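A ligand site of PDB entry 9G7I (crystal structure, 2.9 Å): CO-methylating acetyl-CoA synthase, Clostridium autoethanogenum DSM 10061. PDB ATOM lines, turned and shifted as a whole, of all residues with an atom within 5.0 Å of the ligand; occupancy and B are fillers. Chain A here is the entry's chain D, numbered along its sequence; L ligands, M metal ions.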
ATOM      1  N   ARG A 309      -7.924 -30.184  15.834  1.00  0.00           N
ATOM      2  CA  ARG A 309      -9.274 -29.801  16.341  1.00  0.00           C
ATOM      3  C   ARG A 309      -9.262 -29.807  17.874  1.00  0.00           C
ATOM      4  O   ARG A 309      -9.837 -30.734  18.468  1.00  0.00           O
ATOM      5  CB  ARG A 309     -10.332 -30.760  15.788  1.00  0.00           C
ATOM      6  CG  ARG A 309     -10.455 -30.726  14.274  1.00  0.00           C
ATOM      7  CD  ARG A 309     -10.989 -29.383  13.798  1.00  0.00           C
ATOM      8  NE  ARG A 309     -11.134 -29.330  12.350  1.00  0.00           N
ATOM      9  CZ  ARG A 309     -11.487 -28.229  11.705  1.00  0.00           C
ATOM     10  NH1 ARG A 309     -11.781 -27.150  12.400  1.00  0.00           N
ATOM     11  NH2 ARG A 309     -11.545 -28.219  10.380  1.00  0.00           N
ATOM     12  N   ILE A 310      -8.618 -28.800  18.481  1.00  0.00           N
ATOM     13  CA  ILE A 310      -8.547 -28.695  19.930  1.00  0.00           C
ATOM     14  C   ILE A 310      -9.932 -28.258  20.406  1.00  0.00           C
ATOM     15  O   ILE A 310     -10.269 -27.076  20.310  1.00  0.00           O
ATOM     16  CB  ILE A 310      -7.418 -27.718  20.359  1.00  0.00           C
ATOM     17  CG1 ILE A 310      -6.061 -28.111  19.735  1.00  0.00           C
ATOM     18  CG2 ILE A 310      -7.321 -27.635  21.882  1.00  0.00           C
ATOM     19  CD1 ILE A 310      -5.570 -29.545  19.978  1.00  0.00           C
ATOM     20  N   ARG A 311     -10.736 -29.208  20.870  1.00  0.00           N
ATOM     21  CA  ARG A 311     -12.136 -28.885  21.267  1.00  0.00           C
ATOM     22  C   ARG A 311     -12.198 -28.491  22.748  1.00  0.00           C
ATOM     23  O   ARG A 311     -11.207 -28.724  23.461  1.00  0.00           O
ATOM     24  CB  ARG A 311     -13.058 -30.092  20.996  1.00  0.00           C
ATOM     25  CG  ARG A 311     -12.994 -30.607  19.568  1.00  0.00           C
ATOM     26  CD  ARG A 311     -13.556 -29.650  18.522  1.00  0.00           C
ATOM     27  NE  ARG A 311     -14.172 -30.301  17.382  1.00  0.00           N
ATOM     28  CZ  ARG A 311     -14.190 -29.810  16.149  1.00  0.00           C
ATOM     29  NH1 ARG A 311     -13.752 -28.587  15.906  1.00  0.00           N
ATOM     30  NH2 ARG A 311     -14.634 -30.558  15.153  1.00  0.00           N
ATOM     31  N   LYS A 312     -13.336 -27.937  23.177  1.00  0.00           N
ATOM     32  CA  LYS A 312     -13.502 -27.445  24.577  1.00  0.00           C
ATOM     33  C   LYS A 312     -13.018 -28.456  25.625  1.00  0.00           C
ATOM     34  O   LYS A 312     -12.127 -28.076  26.422  1.00  0.00           O
ATOM     35  CB  LYS A 312     -14.961 -27.075  24.841  1.00  0.00           C
ATOM     36  CG  LYS A 312     -15.989 -27.935  24.109  1.00  0.00           C
ATOM     37  CD  LYS A 312     -16.482 -27.320  22.826  1.00  0.00           C
ATOM     38  CE  LYS A 312     -17.668 -28.057  22.239  1.00  0.00           C
ATOM     39  NZ  LYS A 312     -18.549 -27.147  21.469  1.00  0.00           N
ATOM     40  N   GLU A 318      -7.589 -20.897  26.547  1.00  0.00           N
ATOM     41  CA  GLU A 318      -8.153 -20.279  25.330  1.00  0.00           C
ATOM     42  C   GLU A 318      -7.710 -18.811  25.276  1.00  0.00           C
ATOM     43  O   GLU A 318      -7.643 -18.177  26.346  1.00  0.00           O
ATOM     44  CB  GLU A 318      -9.672 -20.376  25.376  1.00  0.00           C
ATOM     45  CG  GLU A 318     -10.357 -19.842  24.133  1.00  0.00           C
ATOM     46  CD  GLU A 318     -11.826 -20.240  24.065  1.00  0.00           C
ATOM     47  OE1 GLU A 318     -12.439 -20.390  25.142  1.00  0.00           O
ATOM     48  OE2 GLU A 318     -12.334 -20.405  22.956  1.00  0.00           O
ATOM     49  N   GLY A 320      -7.956 -15.141  22.553  1.00  0.00           N
ATOM     50  CA  GLY A 320      -8.574 -14.559  21.342  1.00  0.00           C
ATOM     51  C   GLY A 320     -10.035 -14.966  21.238  1.00  0.00           C
ATOM     52  O   GLY A 320     -10.594 -15.408  22.258  1.00  0.00           O
ATOM     53  N   GLY A 321     -10.612 -14.802  20.054  1.00  0.00           N
ATOM     54  CA  GLY A 321     -12.027 -15.181  19.852  1.00  0.00           C
ATOM     55  C   GLY A 321     -12.956 -14.206  20.552  1.00  0.00           C
ATOM     56  O   GLY A 321     -12.451 -13.225  21.133  1.00  0.00           O
ATOM     57  N   ASN A 322     -14.264 -14.468  20.494  1.00  0.00           N
ATOM     58  CA  ASN A 322     -15.240 -13.615  21.211  1.00  0.00           C
ATOM     59  C   ASN A 322     -15.150 -14.024  22.685  1.00  0.00           C
ATOM     60  O   ASN A 322     -16.201 -14.334  23.272  1.00  0.00           O
ATOM     61  CB  ASN A 322     -16.660 -13.815  20.684  1.00  0.00           C
ATOM     62  CG  ASN A 322     -17.541 -12.592  20.894  1.00  0.00           C
ATOM     63  OD1 ASN A 322     -17.263 -11.526  20.368  1.00  0.00           O
ATOM     64  ND2 ASN A 322     -18.607 -12.761  21.662  1.00  0.00           N
ATOM     65  N   ARG A 383       2.409 -13.102   8.893  1.00  0.00           N
ATOM     66  CA  ARG A 383       1.428 -14.035   8.372  1.00  0.00           C
ATOM     67  C   ARG A 383       1.843 -15.488   8.623  1.00  0.00           C
ATOM     68  O   ARG A 383       0.993 -16.314   8.946  1.00  0.00           O
ATOM     69  CB  ARG A 383       1.191 -13.801   6.858  1.00  0.00           C
ATOM     70  CG  ARG A 383       0.275 -14.810   6.160  1.00  0.00           C
ATOM     71  CD  ARG A 383      -1.184 -14.693   6.560  1.00  0.00           C
ATOM     72  NE  ARG A 383      -1.454 -15.245   7.884  1.00  0.00           N
ATOM     73  CZ  ARG A 383      -2.655 -15.372   8.429  1.00  0.00           C
ATOM     74  NH1 ARG A 383      -3.734 -14.991   7.760  1.00  0.00           N
ATOM     75  NH2 ARG A 383      -2.793 -15.879   9.651  1.00  0.00           N
ATOM     76  N   HIS A 386       0.983 -18.250  11.875  1.00  0.00           N
ATOM     77  CA  HIS A 386      -0.099 -19.230  11.900  1.00  0.00           C
ATOM     78  C   HIS A 386       0.431 -20.604  11.504  1.00  0.00           C
ATOM     79  O   HIS A 386       0.202 -21.594  12.187  1.00  0.00           O
ATOM     80  CB  HIS A 386      -1.243 -18.825  10.960  1.00  0.00           C
ATOM     81  CG  HIS A 386      -2.310 -19.861  10.780  1.00  0.00           C
ATOM     82  ND1 HIS A 386      -3.598 -19.644  11.223  1.00  0.00           N
ATOM     83  CD2 HIS A 386      -2.225 -21.081  10.225  1.00  0.00           C
ATOM     84  CE1 HIS A 386      -4.276 -20.734  10.888  1.00  0.00           C
ATOM     85  NE2 HIS A 386      -3.484 -21.632  10.285  1.00  0.00           N
ATOM     86  N   VAL A 398      -5.523 -19.835  14.989  1.00  0.00           N
ATOM     87  CA  VAL A 398      -6.446 -19.460  13.913  1.00  0.00           C
ATOM     88  C   VAL A 398      -6.636 -17.952  13.932  1.00  0.00           C
ATOM     89  O   VAL A 398      -6.916 -17.396  14.990  1.00  0.00           O
ATOM     90  CB  VAL A 398      -7.808 -20.173  14.085  1.00  0.00           C
ATOM     91  CG1 VAL A 398      -8.787 -19.742  12.998  1.00  0.00           C
ATOM     92  CG2 VAL A 398      -7.648 -21.691  14.099  1.00  0.00           C
ATOM     93  N   GLY A 399      -6.503 -17.301  12.792  1.00  0.00           N
ATOM     94  CA  GLY A 399      -6.706 -15.858  12.673  1.00  0.00           C
ATOM     95  C   GLY A 399      -5.448 -15.092  12.327  1.00  0.00           C
ATOM     96  O   GLY A 399      -4.423 -15.680  11.992  1.00  0.00           O
ATOM     97  N   GLN A 400      -5.521 -13.755  12.409  1.00  0.00           N
ATOM     98  CA  GLN A 400      -4.402 -12.871  12.090  1.00  0.00           C
ATOM     99  C   GLN A 400      -4.549 -11.505  12.768  1.00  0.00           C
ATOM    100  O   GLN A 400      -5.641 -11.135  13.199  1.00  0.00           O
ATOM    101  CB  GLN A 400      -4.319 -12.684  10.569  1.00  0.00           C
ATOM    102  CG  GLN A 400      -5.616 -12.182   9.924  1.00  0.00           C
ATOM    103  CD  GLN A 400      -6.625 -13.284   9.668  1.00  0.00           C
ATOM    104  OE1 GLN A 400      -6.271 -14.420   9.349  1.00  0.00           O
ATOM    105  NE2 GLN A 400      -7.902 -12.961   9.801  1.00  0.00           N
ATOM    106  N   THR A 404      -6.850 -12.932  16.457  1.00  0.00           N
ATOM    107  CA  THR A 404      -6.264 -14.268  16.548  1.00  0.00           C
ATOM    108  C   THR A 404      -7.061 -15.108  17.539  1.00  0.00           C
ATOM    109  O   THR A 404      -7.868 -14.590  18.297  1.00  0.00           O
ATOM    110  CB  THR A 404      -4.774 -14.179  16.946  1.00  0.00           C
ATOM    111  OG1 THR A 404      -4.663 -13.554  18.226  1.00  0.00           O
ATOM    112  CG2 THR A 404      -3.946 -13.444  15.917  1.00  0.00           C
ATOM    113  N   TRP A 405      -6.834 -16.428  17.515  1.00  0.00           N
ATOM    114  CA  TRP A 405      -7.523 -17.370  18.395  1.00  0.00           C
ATOM    115  C   TRP A 405      -6.626 -18.578  18.636  1.00  0.00           C
ATOM    116  O   TRP A 405      -6.491 -19.419  17.760  1.00  0.00           O
ATOM    117  CB  TRP A 405      -8.866 -17.795  17.784  1.00  0.00           C
ATOM    118  CG  TRP A 405      -9.706 -18.675  18.659  1.00  0.00           C
ATOM    119  CD1 TRP A 405      -9.710 -18.725  20.025  1.00  0.00           C
ATOM    120  CD2 TRP A 405     -10.701 -19.605  18.226  1.00  0.00           C
ATOM    121  NE1 TRP A 405     -10.619 -19.655  20.454  1.00  0.00           N
ATOM    122  CE2 TRP A 405     -11.248 -20.203  19.379  1.00  0.00           C
ATOM    123  CE3 TRP A 405     -11.177 -19.997  16.969  1.00  0.00           C
ATOM    124  CZ2 TRP A 405     -12.256 -21.166  19.314  1.00  0.00           C
ATOM    125  CZ3 TRP A 405     -12.164 -20.970  16.908  1.00  0.00           C
ATOM    126  CH2 TRP A 405     -12.686 -21.536  18.063  1.00  0.00           C
ATOM    127  N   ARG A 407      -5.628 -21.980  21.034  1.00  0.00           N
ATOM    128  CA  ARG A 407      -6.237 -22.968  21.906  1.00  0.00           C
ATOM    129  C   ARG A 407      -5.168 -23.996  22.289  1.00  0.00           C
ATOM    130  O   ARG A 407      -4.691 -24.716  21.401  1.00  0.00           O
ATOM    131  CB  ARG A 407      -7.394 -23.683  21.188  1.00  0.00           C
ATOM    132  CG  ARG A 407      -8.608 -22.805  20.950  1.00  0.00           C
ATOM    133  CD  ARG A 407      -9.809 -23.596  20.441  1.00  0.00           C
ATOM    134  NE  ARG A 407     -10.953 -23.502  21.345  1.00  0.00           N
ATOM    135  CZ  ARG A 407     -12.133 -24.097  21.129  1.00  0.00           C
ATOM    136  NH1 ARG A 407     -12.326 -24.821  20.040  1.00  0.00           N
ATOM    137  NH2 ARG A 407     -13.119 -23.946  22.008  1.00  0.00           N
ATOM    138  N   CYS A 488      -4.327 -21.190   3.208  1.00  0.00           N
ATOM    139  CA  CYS A 488      -5.530 -21.693   3.843  1.00  0.00           C
ATOM    140  C   CYS A 488      -6.001 -23.041   3.288  1.00  0.00           C
ATOM    141  O   CYS A 488      -7.116 -23.455   3.616  1.00  0.00           O
ATOM    142  CB  CYS A 488      -6.629 -20.647   3.806  1.00  0.00           C
ATOM    143  SG  CYS A 488      -6.230 -19.140   4.711  1.00  0.00           S
ATOM    144  N   PHE A 491      -6.984 -26.006   5.951  1.00  0.00           N
ATOM    145  CA  PHE A 491      -8.353 -26.120   6.429  1.00  0.00           C
ATOM    146  C   PHE A 491      -9.291 -26.424   5.236  1.00  0.00           C
ATOM    147  O   PHE A 491      -9.920 -27.484   5.215  1.00  0.00           O
ATOM    148  CB  PHE A 491      -8.771 -24.853   7.202  1.00  0.00           C
ATOM    149  CG  PHE A 491      -7.974 -24.616   8.469  1.00  0.00           C
ATOM    150  CD1 PHE A 491      -8.300 -25.256   9.649  1.00  0.00           C
ATOM    151  CD2 PHE A 491      -6.923 -23.716   8.483  1.00  0.00           C
ATOM    152  CE1 PHE A 491      -7.599 -25.001  10.822  1.00  0.00           C
ATOM    153  CE2 PHE A 491      -6.219 -23.469   9.650  1.00  0.00           C
ATOM    154  CZ  PHE A 491      -6.563 -24.107  10.821  1.00  0.00           C
ATOM    155  N   GLY A 575     -12.065 -19.346   5.845  1.00  0.00           N
ATOM    156  CA  GLY A 575     -12.674 -19.220   7.158  1.00  0.00           C
ATOM    157  C   GLY A 575     -12.068 -18.153   8.053  1.00  0.00           C
ATOM    158  O   GLY A 575     -12.517 -17.980   9.190  1.00  0.00           O
ATOM    159  N   CYS A 576     -11.058 -17.444   7.562  1.00  0.00           N
ATOM    160  CA  CYS A 576     -10.398 -16.379   8.317  1.00  0.00           C
ATOM    161  C   CYS A 576     -10.999 -15.003   8.052  1.00  0.00           C
ATOM    162  O   CYS A 576     -10.737 -14.073   8.813  1.00  0.00           O
ATOM    163  CB  CYS A 576      -8.899 -16.392   8.035  1.00  0.00           C
ATOM    164  SG  CYS A 576      -8.497 -16.501   6.269  1.00  0.00           S
ATOM    165  N   ARG A 595     -16.867 -10.083  12.114  1.00  0.00           N
ATOM    166  CA  ARG A 595     -16.739 -11.142  13.111  1.00  0.00           C
ATOM    167  C   ARG A 595     -17.111 -10.702  14.540  1.00  0.00           C
ATOM    168  O   ARG A 595     -17.701 -11.481  15.275  1.00  0.00           O
ATOM    169  CB  ARG A 595     -15.304 -11.704  13.078  1.00  0.00           C
ATOM    170  CG  ARG A 595     -15.180 -13.151  13.565  1.00  0.00           C
ATOM    171  CD  ARG A 595     -13.829 -13.766  13.217  1.00  0.00           C
ATOM    172  NE  ARG A 595     -13.760 -14.209  11.816  1.00  0.00           N
ATOM    173  CZ  ARG A 595     -14.260 -15.353  11.357  1.00  0.00           C
ATOM    174  NH1 ARG A 595     -14.882 -16.197  12.177  1.00  0.00           N
ATOM    175  NH2 ARG A 595     -14.148 -15.664  10.073  1.00  0.00           N
ATOM    176  N   GLY A 608     -21.680 -15.985  12.775  1.00  0.00           N
ATOM    177  CA  GLY A 608     -21.317 -17.391  12.881  1.00  0.00           C
ATOM    178  C   GLY A 608     -22.163 -18.285  12.001  1.00  0.00           C
ATOM    179  O   GLY A 608     -21.656 -19.239  11.402  1.00  0.00           O
HETATM  180  N1  LIG L   1     -13.093 -17.491  15.251  1.00  0.00           N
HETATM  181  C1  LIG L   1     -14.096 -18.263  14.783  1.00  0.00           C
HETATM  182  N2  LIG L   1     -14.886 -18.950  15.651  1.00  0.00           N
HETATM  183  C2  LIG L   1     -14.654 -18.860  16.972  1.00  0.00           C
HETATM  184  C3  LIG L   1     -13.668 -18.100  17.447  1.00  0.00           C
HETATM  185  C4  LIG L   1     -12.875 -17.406  16.556  1.00  0.00           C
HETATM  186  N3  LIG L   1     -11.773 -16.555  16.966  1.00  0.00           N
HETATM  187  N4  LIG L   1     -13.649 -18.189  18.806  1.00  0.00           N
HETATM  188  C5  LIG L   1     -14.627 -18.996  19.219  1.00  0.00           C
HETATM  189  N5  LIG L   1     -15.188 -19.375  18.076  1.00  0.00           N
HETATM  190  C6  LIG L   1     -16.229 -20.202  18.206  1.00  0.00           C
HETATM  191  C7  LIG L   1     -16.611 -20.893  16.882  1.00  0.00           C
HETATM  192  O1  LIG L   1     -17.488 -20.020  16.077  1.00  0.00           O
HETATM  193  C8  LIG L   1     -17.355 -22.136  17.341  1.00  0.00           C
HETATM  194  O2  LIG L   1     -18.764 -21.958  17.205  1.00  0.00           O
HETATM  195  P1  LIG L   1     -19.491 -22.534  15.844  1.00  0.00           P
HETATM  196  O3  LIG L   1     -19.224 -24.011  15.735  1.00  0.00           O
HETATM  197  O4  LIG L   1     -20.984 -22.299  15.933  1.00  0.00           O
HETATM  198  O5  LIG L   1     -18.927 -21.825  14.642  1.00  0.00           O
HETATM  199  C9  LIG L   1     -16.953 -22.270  18.911  1.00  0.00           C
HETATM  200  O6  LIG L   1     -15.932 -21.292  19.079  1.00  0.00           O
HETATM  201  C10 LIG L   1     -16.444 -23.662  19.192  1.00  0.00           C
HETATM  202  O7  LIG L   1     -16.685 -24.467  18.067  1.00  0.00           O
HETATM  203  P2  LIG L   1     -16.643 -26.110  18.205  1.00  0.00           P
HETATM  204  O8  LIG L   1     -17.888 -26.697  17.590  1.00  0.00           O
HETATM  205  O9  LIG L   1     -16.578 -26.502  19.665  1.00  0.00           O
HETATM  206  O10 LIG L   1     -15.309 -26.724  17.452  1.00  0.00           O
HETATM  207  P3  LIG L   1     -13.973 -25.825  17.136  1.00  0.00           P
HETATM  208  O11 LIG L   1     -12.727 -26.590  17.527  1.00  0.00           O
HETATM  209  O12 LIG L   1     -14.014 -24.534  17.918  1.00  0.00           O
HETATM  210  O13 LIG L   1     -13.937 -25.477  15.526  1.00  0.00           O
HETATM  211  C11 LIG L   1     -15.740 -25.199  13.965  1.00  0.00           C
HETATM  212  C12 LIG L   1     -14.889 -24.552  15.055  1.00  0.00           C
HETATM  213  C13 LIG L   1     -16.455 -26.430  14.519  1.00  0.00           C
HETATM  214  C14 LIG L   1     -16.778 -24.177  13.503  1.00  0.00           C
HETATM  215  C15 LIG L   1     -14.824 -25.611  12.805  1.00  0.00           C
HETATM  216  O14 LIG L   1     -14.611 -26.993  12.834  1.00  0.00           O
HETATM  217  C16 LIG L   1     -15.467 -25.221  11.475  1.00  0.00           C
HETATM  218  O15 LIG L   1     -16.363 -25.857  11.030  1.00  0.00           O
HETATM  219  N6  LIG L   1     -14.957 -24.067  10.736  1.00  0.00           N
HETATM  220  C17 LIG L   1     -13.850 -23.286  11.268  1.00  0.00           C
HETATM  221  C18 LIG L   1     -12.522 -23.873  10.758  1.00  0.00           C
HETATM  222  C19 LIG L   1     -11.404 -22.817  10.787  1.00  0.00           C
HETATM  223  O16 LIG L   1     -10.513 -22.923  11.563  1.00  0.00           O
HETATM  224  N7  LIG L   1     -11.437 -21.691   9.860  1.00  0.00           N
HETATM  225  C20 LIG L   1     -10.364 -20.708   9.895  1.00  0.00           C
HETATM  226  C21 LIG L   1      -9.080 -21.389   9.403  1.00  0.00           C
HETATM  227  S1  LIG L   1      -8.205 -20.306   8.239  1.00  0.00           S
HETATM  228  C22 LIG L   1      -7.116 -19.213   9.200  1.00  0.00           C
HETATM  229  O17 LIG L   1      -7.440 -18.858  10.276  1.00  0.00           O
HETATM  230  C23 LIG L   1      -5.768 -18.763   8.625  1.00  0.00           C
HETATM  231 NI    NI M   1      -7.809 -18.008   4.833  1.00  0.00          NI
HETATM  232 NI    NI M   2     -10.483 -17.810   5.824  1.00  0.00          NI
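NH1 of Arg 407 is in hydrogen-bond range of O of Ile 310 (3.1 Å). The guanidinium group (NH2) of Arg 407 lies within salt-bridge range of the side-chain carboxylate (OE2) of Glu 318 (3.7 Å). O of Gly 399 is in hydrogen-bond range of NH2 of Arg 383. The backbone NH of Trp 405 is in hydrogen-bond range of the backbone carbonyl oxygen of Val 398, at 2.7 Å. The indole nitrogen of Trp 405 lies within hydrogen-bond range of the side-chain carboxylate of Glu 318 (3.1 Å). The backbone NH (N) of Gly 321 lies within hydrogen-bond range of the backbone carbonyl oxygen (O) of Thr 404 (3.3 Å). The guanidinium group (NH2) of Arg 595 sits at hydrogen-bond distance from the backbone carbonyl oxygen (O) of Gly 575 (3.0 Å). The side-chain amide nitrogen (NE2) of Gln 400 lies within hydrogen-bond range of the backbone carbonyl oxygen (O) of Cys 576.
Merely in contact with the ligand: Ile 310, Gly 321, His 386, Val 398, Trp 405, Cys 488, Phe 491, Gly 575, Cys 576 and Arg 595. Hydrophobic or aromatic side chains that line the ligand: His 386, Val 398, Trp 405 and Phe 491. Of the 22 residues printed, 15 come within 4 Å of the ligand.
An oxygen (O12) of the ligand lies within salt-bridge range of the guanidinium group of Arg 407 (2.7 Å). NZ of Lys 312 is in salt-bridge range of O9 of the ligand. The guanidinium group of Arg 311 is in salt-bridge range of an oxygen (O11) of the ligand (2.8 Å). NH1 of Arg 309 lies within hydrogen-bond range of O14 of the ligand (2.9 Å). The backbone NH (N) of Gly 399 is in hydrogen-bond range of an oxygen (O17) of the ligand (3.1 Å).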
